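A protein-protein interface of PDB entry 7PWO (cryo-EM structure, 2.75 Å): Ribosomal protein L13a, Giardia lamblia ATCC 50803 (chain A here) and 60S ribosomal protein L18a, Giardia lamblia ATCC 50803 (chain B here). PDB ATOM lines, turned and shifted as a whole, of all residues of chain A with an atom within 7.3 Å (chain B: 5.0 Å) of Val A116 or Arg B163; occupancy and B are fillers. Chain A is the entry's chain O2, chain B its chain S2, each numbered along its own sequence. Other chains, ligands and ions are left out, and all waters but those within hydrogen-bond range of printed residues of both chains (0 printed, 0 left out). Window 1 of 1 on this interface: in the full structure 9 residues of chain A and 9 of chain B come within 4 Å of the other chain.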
ATOM      1  N   VAL A   5     -28.097  31.431 -29.695  1.00  0.00           N
ATOM      2  CA  VAL A   5     -27.133  32.379 -29.145  1.00  0.00           C
ATOM      3  C   VAL A   5     -26.036  31.579 -28.463  1.00  0.00           C
ATOM      4  O   VAL A   5     -26.311  30.794 -27.550  1.00  0.00           O
ATOM      5  CB  VAL A   5     -27.794  33.359 -28.166  1.00  0.00           C
ATOM      6  CG1 VAL A   5     -26.754  34.277 -27.562  1.00  0.00           C
ATOM      7  CG2 VAL A   5     -28.870  34.147 -28.863  1.00  0.00           C
ATOM      8  N   ILE A   6     -24.796  31.770 -28.898  1.00  0.00           N
ATOM      9  CA  ILE A   6     -23.687  30.937 -28.449  1.00  0.00           C
ATOM     10  C   ILE A   6     -22.679  31.806 -27.721  1.00  0.00           C
ATOM     11  O   ILE A   6     -22.246  32.836 -28.246  1.00  0.00           O
ATOM     12  CB  ILE A   6     -23.020  30.194 -29.620  1.00  0.00           C
ATOM     13  CG1 ILE A   6     -24.042  29.325 -30.354  1.00  0.00           C
ATOM     14  CG2 ILE A   6     -21.868  29.330 -29.122  1.00  0.00           C
ATOM     15  CD1 ILE A   6     -23.499  28.674 -31.591  1.00  0.00           C
ATOM     16  N   ASP A   7     -22.299  31.379 -26.522  1.00  0.00           N
ATOM     17  CA  ASP A   7     -21.292  32.058 -25.720  1.00  0.00           C
ATOM     18  C   ASP A   7     -19.916  31.521 -26.100  1.00  0.00           C
ATOM     19  O   ASP A   7     -19.627  30.340 -25.889  1.00  0.00           O
ATOM     20  CB  ASP A   7     -21.604  31.846 -24.239  1.00  0.00           C
ATOM     21  CG  ASP A   7     -20.433  32.117 -23.342  1.00  0.00           C
ATOM     22  OD1 ASP A   7     -19.645  33.037 -23.629  1.00  0.00           O
ATOM     23  OD2 ASP A   7     -20.301  31.397 -22.333  1.00  0.00           O
ATOM     24  N   CYS A   8     -19.070  32.387 -26.657  1.00  0.00           N
ATOM     25  CA  CYS A   8     -17.833  31.953 -27.291  1.00  0.00           C
ATOM     26  C   CYS A   8     -16.671  31.809 -26.317  1.00  0.00           C
ATOM     27  O   CYS A   8     -15.545  31.570 -26.754  1.00  0.00           O
ATOM     28  CB  CYS A   8     -17.448  32.908 -28.420  1.00  0.00           C
ATOM     29  SG  CYS A   8     -18.567  32.912 -29.828  1.00  0.00           S
ATOM     30  N   LYS A   9     -16.911  31.952 -25.019  1.00  0.00           N
ATOM     31  CA  LYS A   9     -15.906  31.588 -24.032  1.00  0.00           C
ATOM     32  C   LYS A   9     -15.605  30.096 -24.114  1.00  0.00           C
ATOM     33  O   LYS A   9     -16.519  29.271 -24.090  1.00  0.00           O
ATOM     34  CB  LYS A   9     -16.407  31.929 -22.636  1.00  0.00           C
ATOM     35  CG  LYS A   9     -15.408  31.686 -21.535  1.00  0.00           C
ATOM     36  CD  LYS A   9     -15.992  32.124 -20.214  1.00  0.00           C
ATOM     37  CE  LYS A   9     -15.038  31.886 -19.076  1.00  0.00           C
ATOM     38  NZ  LYS A   9     -15.650  32.320 -17.803  1.00  0.00           N
ATOM     39  N   HIS A  11     -14.233  28.182 -26.541  1.00  0.00           N
ATOM     40  CA  HIS A  11     -14.321  27.442 -27.792  1.00  0.00           C
ATOM     41  C   HIS A  11     -13.126  27.687 -28.703  1.00  0.00           C
ATOM     42  O   HIS A  11     -12.498  28.744 -28.673  1.00  0.00           O
ATOM     43  CB  HIS A  11     -15.604  27.805 -28.540  1.00  0.00           C
ATOM     44  CG  HIS A  11     -16.851  27.512 -27.772  1.00  0.00           C
ATOM     45  ND1 HIS A  11     -17.120  28.084 -26.550  1.00  0.00           N
ATOM     46  CD2 HIS A  11     -17.896  26.702 -28.046  1.00  0.00           C
ATOM     47  CE1 HIS A  11     -18.276  27.636 -26.104  1.00  0.00           C
ATOM     48  NE2 HIS A  11     -18.771  26.802 -26.996  1.00  0.00           N
ATOM     49  N   LEU A  16     -15.646  25.901 -33.833  1.00  0.00           N
ATOM     50  CA  LEU A  16     -16.876  26.673 -33.725  1.00  0.00           C
ATOM     51  C   LEU A  16     -17.287  27.261 -35.071  1.00  0.00           C
ATOM     52  O   LEU A  16     -18.476  27.292 -35.400  1.00  0.00           O
ATOM     53  CB  LEU A  16     -16.718  27.782 -32.688  1.00  0.00           C
ATOM     54  CG  LEU A  16     -18.065  28.321 -32.210  1.00  0.00           C
ATOM     55  CD1 LEU A  16     -18.844  27.218 -31.511  1.00  0.00           C
ATOM     56  CD2 LEU A  16     -17.883  29.514 -31.315  1.00  0.00           C
ATOM     57  N   ALA A  18     -16.780  26.061 -38.091  1.00  0.00           N
ATOM     58  CA  ALA A  18     -17.374  25.015 -38.914  1.00  0.00           C
ATOM     59  C   ALA A  18     -18.814  24.747 -38.498  1.00  0.00           C
ATOM     60  O   ALA A  18     -19.720  24.669 -39.350  1.00  0.00           O
ATOM     61  CB  ALA A  18     -16.534  23.741 -38.832  1.00  0.00           C
ATOM     62  N   ILE A  19     -19.054  24.641 -37.182  1.00  0.00           N
ATOM     63  CA  ILE A  19     -20.425  24.436 -36.706  1.00  0.00           C
ATOM     64  C   ILE A  19     -21.341  25.570 -37.168  1.00  0.00           C
ATOM     65  O   ILE A  19     -22.415  25.332 -37.736  1.00  0.00           O
ATOM     66  CB  ILE A  19     -20.453  24.286 -35.175  1.00  0.00           C
ATOM     67  CG1 ILE A  19     -19.940  22.908 -34.760  1.00  0.00           C
ATOM     68  CG2 ILE A  19     -21.859  24.475 -34.649  1.00  0.00           C
ATOM     69  CD1 ILE A  19     -19.719  22.772 -33.285  1.00  0.00           C
ATOM     70  N   VAL A  20     -20.928  26.816 -36.931  1.00  0.00           N
ATOM     71  CA  VAL A  20     -21.780  27.965 -37.231  1.00  0.00           C
ATOM     72  C   VAL A  20     -22.101  28.024 -38.719  1.00  0.00           C
ATOM     73  O   VAL A  20     -23.233  28.327 -39.106  1.00  0.00           O
ATOM     74  CB  VAL A  20     -21.120  29.267 -36.735  1.00  0.00           C
ATOM     75  CG1 VAL A  20     -21.944  30.484 -37.139  1.00  0.00           C
ATOM     76  CG2 VAL A  20     -20.961  29.243 -35.234  1.00  0.00           C
ATOM     77  N   LYS A  22     -22.272  25.510 -40.966  1.00  0.00           N
ATOM     78  CA  LYS A  22     -23.286  24.528 -41.353  1.00  0.00           C
ATOM     79  C   LYS A  22     -24.672  24.935 -40.849  1.00  0.00           C
ATOM     80  O   LYS A  22     -25.676  24.839 -41.581  1.00  0.00           O
ATOM     81  CB  LYS A  22     -22.905  23.142 -40.833  1.00  0.00           C
ATOM     82  CG  LYS A  22     -23.650  22.011 -41.523  1.00  0.00           C
ATOM     83  CD  LYS A  22     -23.316  21.982 -42.991  1.00  0.00           C
ATOM     84  CE  LYS A  22     -23.482  20.603 -43.584  1.00  0.00           C
ATOM     85  NZ  LYS A  22     -23.549  20.661 -45.057  1.00  0.00           N
ATOM     86  N   GLU A  23     -24.740  25.430 -39.613  1.00  0.00           N
ATOM     87  CA  GLU A  23     -26.023  25.835 -39.054  1.00  0.00           C
ATOM     88  C   GLU A  23     -26.636  26.976 -39.853  1.00  0.00           C
ATOM     89  O   GLU A  23     -27.850  27.001 -40.074  1.00  0.00           O
ATOM     90  CB  GLU A  23     -25.857  26.234 -37.589  1.00  0.00           C
ATOM     91  CG  GLU A  23     -25.640  25.070 -36.635  1.00  0.00           C
ATOM     92  CD  GLU A  23     -26.729  24.008 -36.704  1.00  0.00           C
ATOM     93  OE1 GLU A  23     -26.508  22.963 -37.346  1.00  0.00           O
ATOM     94  OE2 GLU A  23     -27.802  24.208 -36.104  1.00  0.00           O
ATOM     95  N   ARG A 114     -28.217  31.453 -23.646  1.00  0.00           N
ATOM     96  CA  ARG A 114     -27.000  30.991 -24.289  1.00  0.00           C
ATOM     97  C   ARG A 114     -26.822  29.482 -24.197  1.00  0.00           C
ATOM     98  O   ARG A 114     -27.315  28.825 -23.282  1.00  0.00           O
ATOM     99  CB  ARG A 114     -25.762  31.693 -23.724  1.00  0.00           C
ATOM    100  CG  ARG A 114     -25.531  33.076 -24.290  1.00  0.00           C
ATOM    101  CD  ARG A 114     -26.317  34.205 -23.678  1.00  0.00           C
ATOM    102  NE  ARG A 114     -25.954  34.448 -22.290  1.00  0.00           N
ATOM    103  CZ  ARG A 114     -26.663  35.213 -21.468  1.00  0.00           C
ATOM    104  NH1 ARG A 114     -27.750  35.819 -21.912  1.00  0.00           N
ATOM    105  NH2 ARG A 114     -26.273  35.380 -20.214  1.00  0.00           N
ATOM    106  N   VAL A 115     -26.099  28.944 -25.180  1.00  0.00           N
ATOM    107  CA  VAL A 115     -25.740  27.534 -25.244  1.00  0.00           C
ATOM    108  C   VAL A 115     -24.247  27.440 -25.520  1.00  0.00           C
ATOM    109  O   VAL A 115     -23.583  28.434 -25.808  1.00  0.00           O
ATOM    110  CB  VAL A 115     -26.536  26.770 -26.321  1.00  0.00           C
ATOM    111  CG1 VAL A 115     -27.964  26.595 -25.887  1.00  0.00           C
ATOM    112  CG2 VAL A 115     -26.467  27.486 -27.650  1.00  0.00           C
ATOM    113  N   VAL A 116     -23.716  26.219 -25.426  1.00  0.00           N
ATOM    114  CA  VAL A 116     -22.313  25.951 -25.716  1.00  0.00           C
ATOM    115  C   VAL A 116     -22.226  24.757 -26.660  1.00  0.00           C
ATOM    116  O   VAL A 116     -23.225  24.117 -26.983  1.00  0.00           O
ATOM    117  CB  VAL A 116     -21.472  25.692 -24.446  1.00  0.00           C
ATOM    118  CG1 VAL A 116     -21.478  26.903 -23.540  1.00  0.00           C
ATOM    119  CG2 VAL A 116     -21.933  24.458 -23.733  1.00  0.00           C
ATOM    120  N   CYS A 117     -21.005  24.484 -27.119  1.00  0.00           N
ATOM    121  CA  CYS A 117     -20.711  23.384 -28.034  1.00  0.00           C
ATOM    122  C   CYS A 117     -19.502  22.640 -27.487  1.00  0.00           C
ATOM    123  O   CYS A 117     -18.370  22.866 -27.931  1.00  0.00           O
ATOM    124  CB  CYS A 117     -20.439  23.896 -29.450  1.00  0.00           C
ATOM    125  SG  CYS A 117     -21.879  24.417 -30.384  1.00  0.00           S
ATOM    126  N   PRO A 118     -19.700  21.753 -26.509  1.00  0.00           N
ATOM    127  CA  PRO A 118     -18.546  21.158 -25.815  1.00  0.00           C
ATOM    128  C   PRO A 118     -17.609  20.372 -26.715  1.00  0.00           C
ATOM    129  O   PRO A 118     -16.414  20.280 -26.411  1.00  0.00           O
ATOM    130  CB  PRO A 118     -19.195  20.263 -24.750  1.00  0.00           C
ATOM    131  CG  PRO A 118     -20.642  20.247 -25.043  1.00  0.00           C
ATOM    132  CD  PRO A 118     -20.981  21.402 -25.877  1.00  0.00           C
ATOM    133  N   SER A 119     -18.093  19.814 -27.820  1.00  0.00           N
ATOM    134  CA  SER A 119     -17.194  19.084 -28.703  1.00  0.00           C
ATOM    135  C   SER A 119     -16.223  20.000 -29.449  1.00  0.00           C
ATOM    136  O   SER A 119     -15.392  19.504 -30.211  1.00  0.00           O
ATOM    137  CB  SER A 119     -18.010  18.234 -29.679  1.00  0.00           C
ATOM    138  OG  SER A 119     -18.767  19.038 -30.563  1.00  0.00           O
ATOM    139  N   ALA A 120     -16.295  21.312 -29.225  1.00  0.00           N
ATOM    140  CA  ALA A 120     -15.360  22.276 -29.788  1.00  0.00           C
ATOM    141  C   ALA A 120     -14.760  23.179 -28.717  1.00  0.00           C
ATOM    142  O   ALA A 120     -14.187  24.217 -29.046  1.00  0.00           O
ATOM    143  CB  ALA A 120     -16.039  23.125 -30.860  1.00  0.00           C
ATOM    144  N   MET A 121     -14.876  22.810 -27.447  1.00  0.00           N
ATOM    145  CA  MET A 121     -14.282  23.588 -26.373  1.00  0.00           C
ATOM    146  C   MET A 121     -12.881  23.068 -26.058  1.00  0.00           C
ATOM    147  O   MET A 121     -12.606  21.870 -26.153  1.00  0.00           O
ATOM    148  CB  MET A 121     -15.170  23.562 -25.126  1.00  0.00           C
ATOM    149  CG  MET A 121     -16.316  24.557 -25.170  1.00  0.00           C
ATOM    150  SD  MET A 121     -17.619  24.307 -23.949  1.00  0.00           S
ATOM    151  CE  MET A 121     -17.271  25.689 -22.870  1.00  0.00           C
ATOM    152  N   TYR A 123     -10.948  22.768 -23.352  1.00  0.00           N
ATOM    153  CA  TYR A 123     -10.664  21.835 -22.266  1.00  0.00           C
ATOM    154  C   TYR A 123     -11.008  20.394 -22.622  1.00  0.00           C
ATOM    155  O   TYR A 123     -10.586  19.476 -21.915  1.00  0.00           O
ATOM    156  CB  TYR A 123     -11.392  22.266 -20.989  1.00  0.00           C
ATOM    157  CG  TYR A 123     -12.835  21.845 -20.890  1.00  0.00           C
ATOM    158  CD1 TYR A 123     -13.826  22.533 -21.569  1.00  0.00           C
ATOM    159  CD2 TYR A 123     -13.208  20.764 -20.116  1.00  0.00           C
ATOM    160  CE1 TYR A 123     -15.142  22.151 -21.489  1.00  0.00           C
ATOM    161  CE2 TYR A 123     -14.534  20.374 -20.033  1.00  0.00           C
ATOM    162  CZ  TYR A 123     -15.491  21.074 -20.719  1.00  0.00           C
ATOM    163  OH  TYR A 123     -16.810  20.705 -20.640  1.00  0.00           O
ATOM    164  N   ALA B 159     -21.007  14.419 -26.683  1.00  0.00           N
ATOM    165  CA  ALA B 159     -21.239  15.700 -27.349  1.00  0.00           C
ATOM    166  C   ALA B 159     -21.464  15.531 -28.845  1.00  0.00           C
ATOM    167  O   ALA B 159     -22.235  16.292 -29.448  1.00  0.00           O
ATOM    168  CB  ALA B 159     -20.066  16.644 -27.099  1.00  0.00           C
ATOM    169  N   ARG B 160     -20.810  14.529 -29.448  1.00  0.00           N
ATOM    170  CA  ARG B 160     -20.947  14.251 -30.880  1.00  0.00           C
ATOM    171  C   ARG B 160     -22.399  14.188 -31.329  1.00  0.00           C
ATOM    172  O   ARG B 160     -22.694  14.428 -32.503  1.00  0.00           O
ATOM    173  CB  ARG B 160     -20.260  12.925 -31.229  1.00  0.00           C
ATOM    174  CG  ARG B 160     -20.350  12.513 -32.697  1.00  0.00           C
ATOM    175  CD  ARG B 160     -19.591  11.222 -32.981  1.00  0.00           C
ATOM    176  NE  ARG B 160     -18.255  11.453 -33.517  1.00  0.00           N
ATOM    177  CZ  ARG B 160     -17.139  11.026 -32.935  1.00  0.00           C
ATOM    178  NH1 ARG B 160     -17.201  10.339 -31.801  1.00  0.00           N
ATOM    179  NH2 ARG B 160     -15.960  11.286 -33.488  1.00  0.00           N
ATOM    180  N   THR B 161     -23.306  13.854 -30.433  1.00  0.00           N
ATOM    181  CA  THR B 161     -24.731  13.841 -30.714  1.00  0.00           C
ATOM    182  C   THR B 161     -25.489  14.886 -29.918  1.00  0.00           C
ATOM    183  O   THR B 161     -26.454  15.452 -30.429  1.00  0.00           O
ATOM    184  CB  THR B 161     -25.299  12.443 -30.430  1.00  0.00           C
ATOM    185  OG1 THR B 161     -24.640  11.485 -31.266  1.00  0.00           O
ATOM    186  CG2 THR B 161     -26.781  12.383 -30.682  1.00  0.00           C
ATOM    187  N   ALA B 162     -25.061  15.176 -28.692  1.00  0.00           N
ATOM    188  CA  ALA B 162     -25.534  16.346 -27.954  1.00  0.00           C
ATOM    189  C   ALA B 162     -24.705  17.573 -28.344  1.00  0.00           C
ATOM    190  O   ALA B 162     -23.989  18.173 -27.547  1.00  0.00           O
ATOM    191  CB  ALA B 162     -25.482  16.075 -26.457  1.00  0.00           C
ATOM    192  N   ARG B 163     -24.816  17.903 -29.633  1.00  0.00           N
ATOM    193  CA  ARG B 163     -24.131  19.041 -30.248  1.00  0.00           C
ATOM    194  C   ARG B 163     -24.322  20.365 -29.501  1.00  0.00           C
ATOM    195  O   ARG B 163     -23.381  21.157 -29.395  1.00  0.00           O
ATOM    196  CB  ARG B 163     -24.611  19.177 -31.691  1.00  0.00           C
ATOM    197  CG  ARG B 163     -24.011  20.328 -32.448  1.00  0.00           C
ATOM    198  CD  ARG B 163     -24.645  20.429 -33.801  1.00  0.00           C
ATOM    199  NE  ARG B 163     -24.092  19.464 -34.739  1.00  0.00           N
ATOM    200  CZ  ARG B 163     -23.477  19.797 -35.866  1.00  0.00           C
ATOM    201  NH1 ARG B 163     -23.353  21.071 -36.204  1.00  0.00           N
ATOM    202  NH2 ARG B 163     -23.003  18.853 -36.660  1.00  0.00           N
ATOM    203  N   PHE B 164     -25.530  20.650 -29.021  1.00  0.00           N
ATOM    204  CA  PHE B 164     -25.792  21.863 -28.250  1.00  0.00           C
ATOM    205  C   PHE B 164     -26.282  21.486 -26.861  1.00  0.00           C
ATOM    206  O   PHE B 164     -27.030  20.519 -26.706  1.00  0.00           O
ATOM    207  CB  PHE B 164     -26.844  22.765 -28.910  1.00  0.00           C
ATOM    208  CG  PHE B 164     -26.474  23.252 -30.277  1.00  0.00           C
ATOM    209  CD1 PHE B 164     -26.790  22.511 -31.399  1.00  0.00           C
ATOM    210  CD2 PHE B 164     -25.811  24.453 -30.445  1.00  0.00           C
ATOM    211  CE1 PHE B 164     -26.463  22.966 -32.658  1.00  0.00           C
ATOM    212  CE2 PHE B 164     -25.478  24.898 -31.703  1.00  0.00           C
ATOM    213  CZ  PHE B 164     -25.802  24.154 -32.808  1.00  0.00           C
ATOM    214  N   GLN B 165     -25.864  22.250 -25.850  1.00  0.00           N
ATOM    215  CA  GLN B 165     -26.210  21.971 -24.460  1.00  0.00           C
ATOM    216  C   GLN B 165     -26.454  23.289 -23.733  1.00  0.00           C
ATOM    217  O   GLN B 165     -26.271  24.365 -24.301  1.00  0.00           O
ATOM    218  CB  GLN B 165     -25.114  21.133 -23.798  1.00  0.00           C
ATOM    219  CG  GLN B 165     -25.010  19.735 -24.387  1.00  0.00           C
ATOM    220  CD  GLN B 165     -23.930  18.907 -23.752  1.00  0.00           C
ATOM    221  OE1 GLN B 165     -23.196  19.382 -22.897  1.00  0.00           O
ATOM    222  NE2 GLN B 165     -23.811  17.665 -24.183  1.00  0.00           N
ATOM    223  N   ARG B 167     -24.932  23.858 -20.580  1.00  0.00           N
ATOM    224  CA  ARG B 167     -23.772  24.124 -19.736  1.00  0.00           C
ATOM    225  C   ARG B 167     -22.612  23.287 -20.239  1.00  0.00           C
ATOM    226  O   ARG B 167     -22.804  22.290 -20.934  1.00  0.00           O
ATOM    227  CB  ARG B 167     -24.038  23.811 -18.258  1.00  0.00           C
ATOM    228  CG  ARG B 167     -23.916  22.327 -17.887  1.00  0.00           C
ATOM    229  CD  ARG B 167     -25.071  21.518 -18.455  1.00  0.00           C
ATOM    230  NE  ARG B 167     -25.025  20.103 -18.110  1.00  0.00           N
ATOM    231  CZ  ARG B 167     -24.402  19.189 -18.843  1.00  0.00           C
ATOM    232  NH1 ARG B 167     -23.774  19.548 -19.949  1.00  0.00           N
ATOM    233  NH2 ARG B 167     -24.407  17.917 -18.478  1.00  0.00           N
ATOM    234  N   ALA B 168     -21.407  23.684 -19.860  1.00  0.00           N
ATOM    235  CA  ALA B 168     -20.241  22.883 -20.186  1.00  0.00           C
ATOM    236  C   ALA B 168     -20.164  21.706 -19.220  1.00  0.00           C
ATOM    237  O   ALA B 168     -20.040  21.921 -18.011  1.00  0.00           O
ATOM    238  CB  ALA B 168     -18.977  23.726 -20.125  1.00  0.00           C
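N of Val A116 lies within hydrogen-bond range of O of Gln B165, 3.4 Å away.
OE1 of Glu A23 lies within salt-bridge range of NH1 of Arg B163 (3.9 Å).
O of Arg B163 is in hydrogen-bond range of SG of Cys A117 (3.7 Å).
Lys A9 touches none of the printed residues of chain B.
Val A20 touches none of the printed residues of chain B.
Printed residues of chain B within 4 Å of Val A115: Gln B165 (3.2 Å).
Printed residues of chain B within 4 Å of Tyr A123: Ala B168 (3.8 Å).
Arg B163 touches just these residues of chain A: Glu A23, Val A116 and Cys A117.
Printed residues of chain A within 4 Å of Gln B165: Val A115 (3.2 Å), Val A116 (3.4 Å) and Pro A118 (3.4 Å).
The nearest printed residue of chain B that does not touch Val A116 is Ala B162 (6.0 Å).
The nearest residue of chain A that does not touch Arg B163 is Ile A19 (4.03 Å).
Printed residues of chain B that touch a printed residue of chain A: Ala B159, Arg B163, Phe B164, Gln B165, Arg B167 and Ala B168.
Hydrophobic or aromatic side chains of chain B within 4 Å of the printed part of chain A: Ala B159, Phe B164 and Ala B168.
Hydrophobic or aromatic side chains of chain A that line the printed part of chain B: Val A115, Val A116, Pro A118, Met A121 and Tyr A123.
Among the printed residues, pairs that only touch across the chains: Val A115 with Gln B165 (3.2 Å), Pro A118 with Gln B165 (3.4 Å), Val A116 with Phe B164 (3.6 Å), Val A116 with Arg B167 (3.6 Å), Ser A119 with Ala B159 (3.7 Å), Tyr A123 with Ala B168 (3.8 Å), Met A121 with Ala B168 (3.8 Å), Val A116 with Arg B163 (3.8 Å), Glu A23 with Phe B164 (3.9 Å), Cys A117 with Phe B164 (3.9 Å) and Val A116 with Ala B168 (3.98 Å).
The backbone carbonyl oxygen (O) of Val A5 lies within hydrogen-bond range of the backbone NH (N) of Val A115, at 3.0 Å.
The side-chain amide oxygen of Gln B165 sits at hydrogen-bond distance from the guanidinium group of Arg B167.
A ring nitrogen (NE2) of His A11 lies within hydrogen-bond range of the backbone NH (N) of Cys A117 (3.2 Å).
The backbone carbonyl oxygen of Ala B162 sits close to the side-chain amide nitrogen of Gln B165 (3.4 Å).
The backbone NH (N) of Asp A7 is in hydrogen-bond range of the backbone carbonyl oxygen (O) of Val A115, 3.3 Å away.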
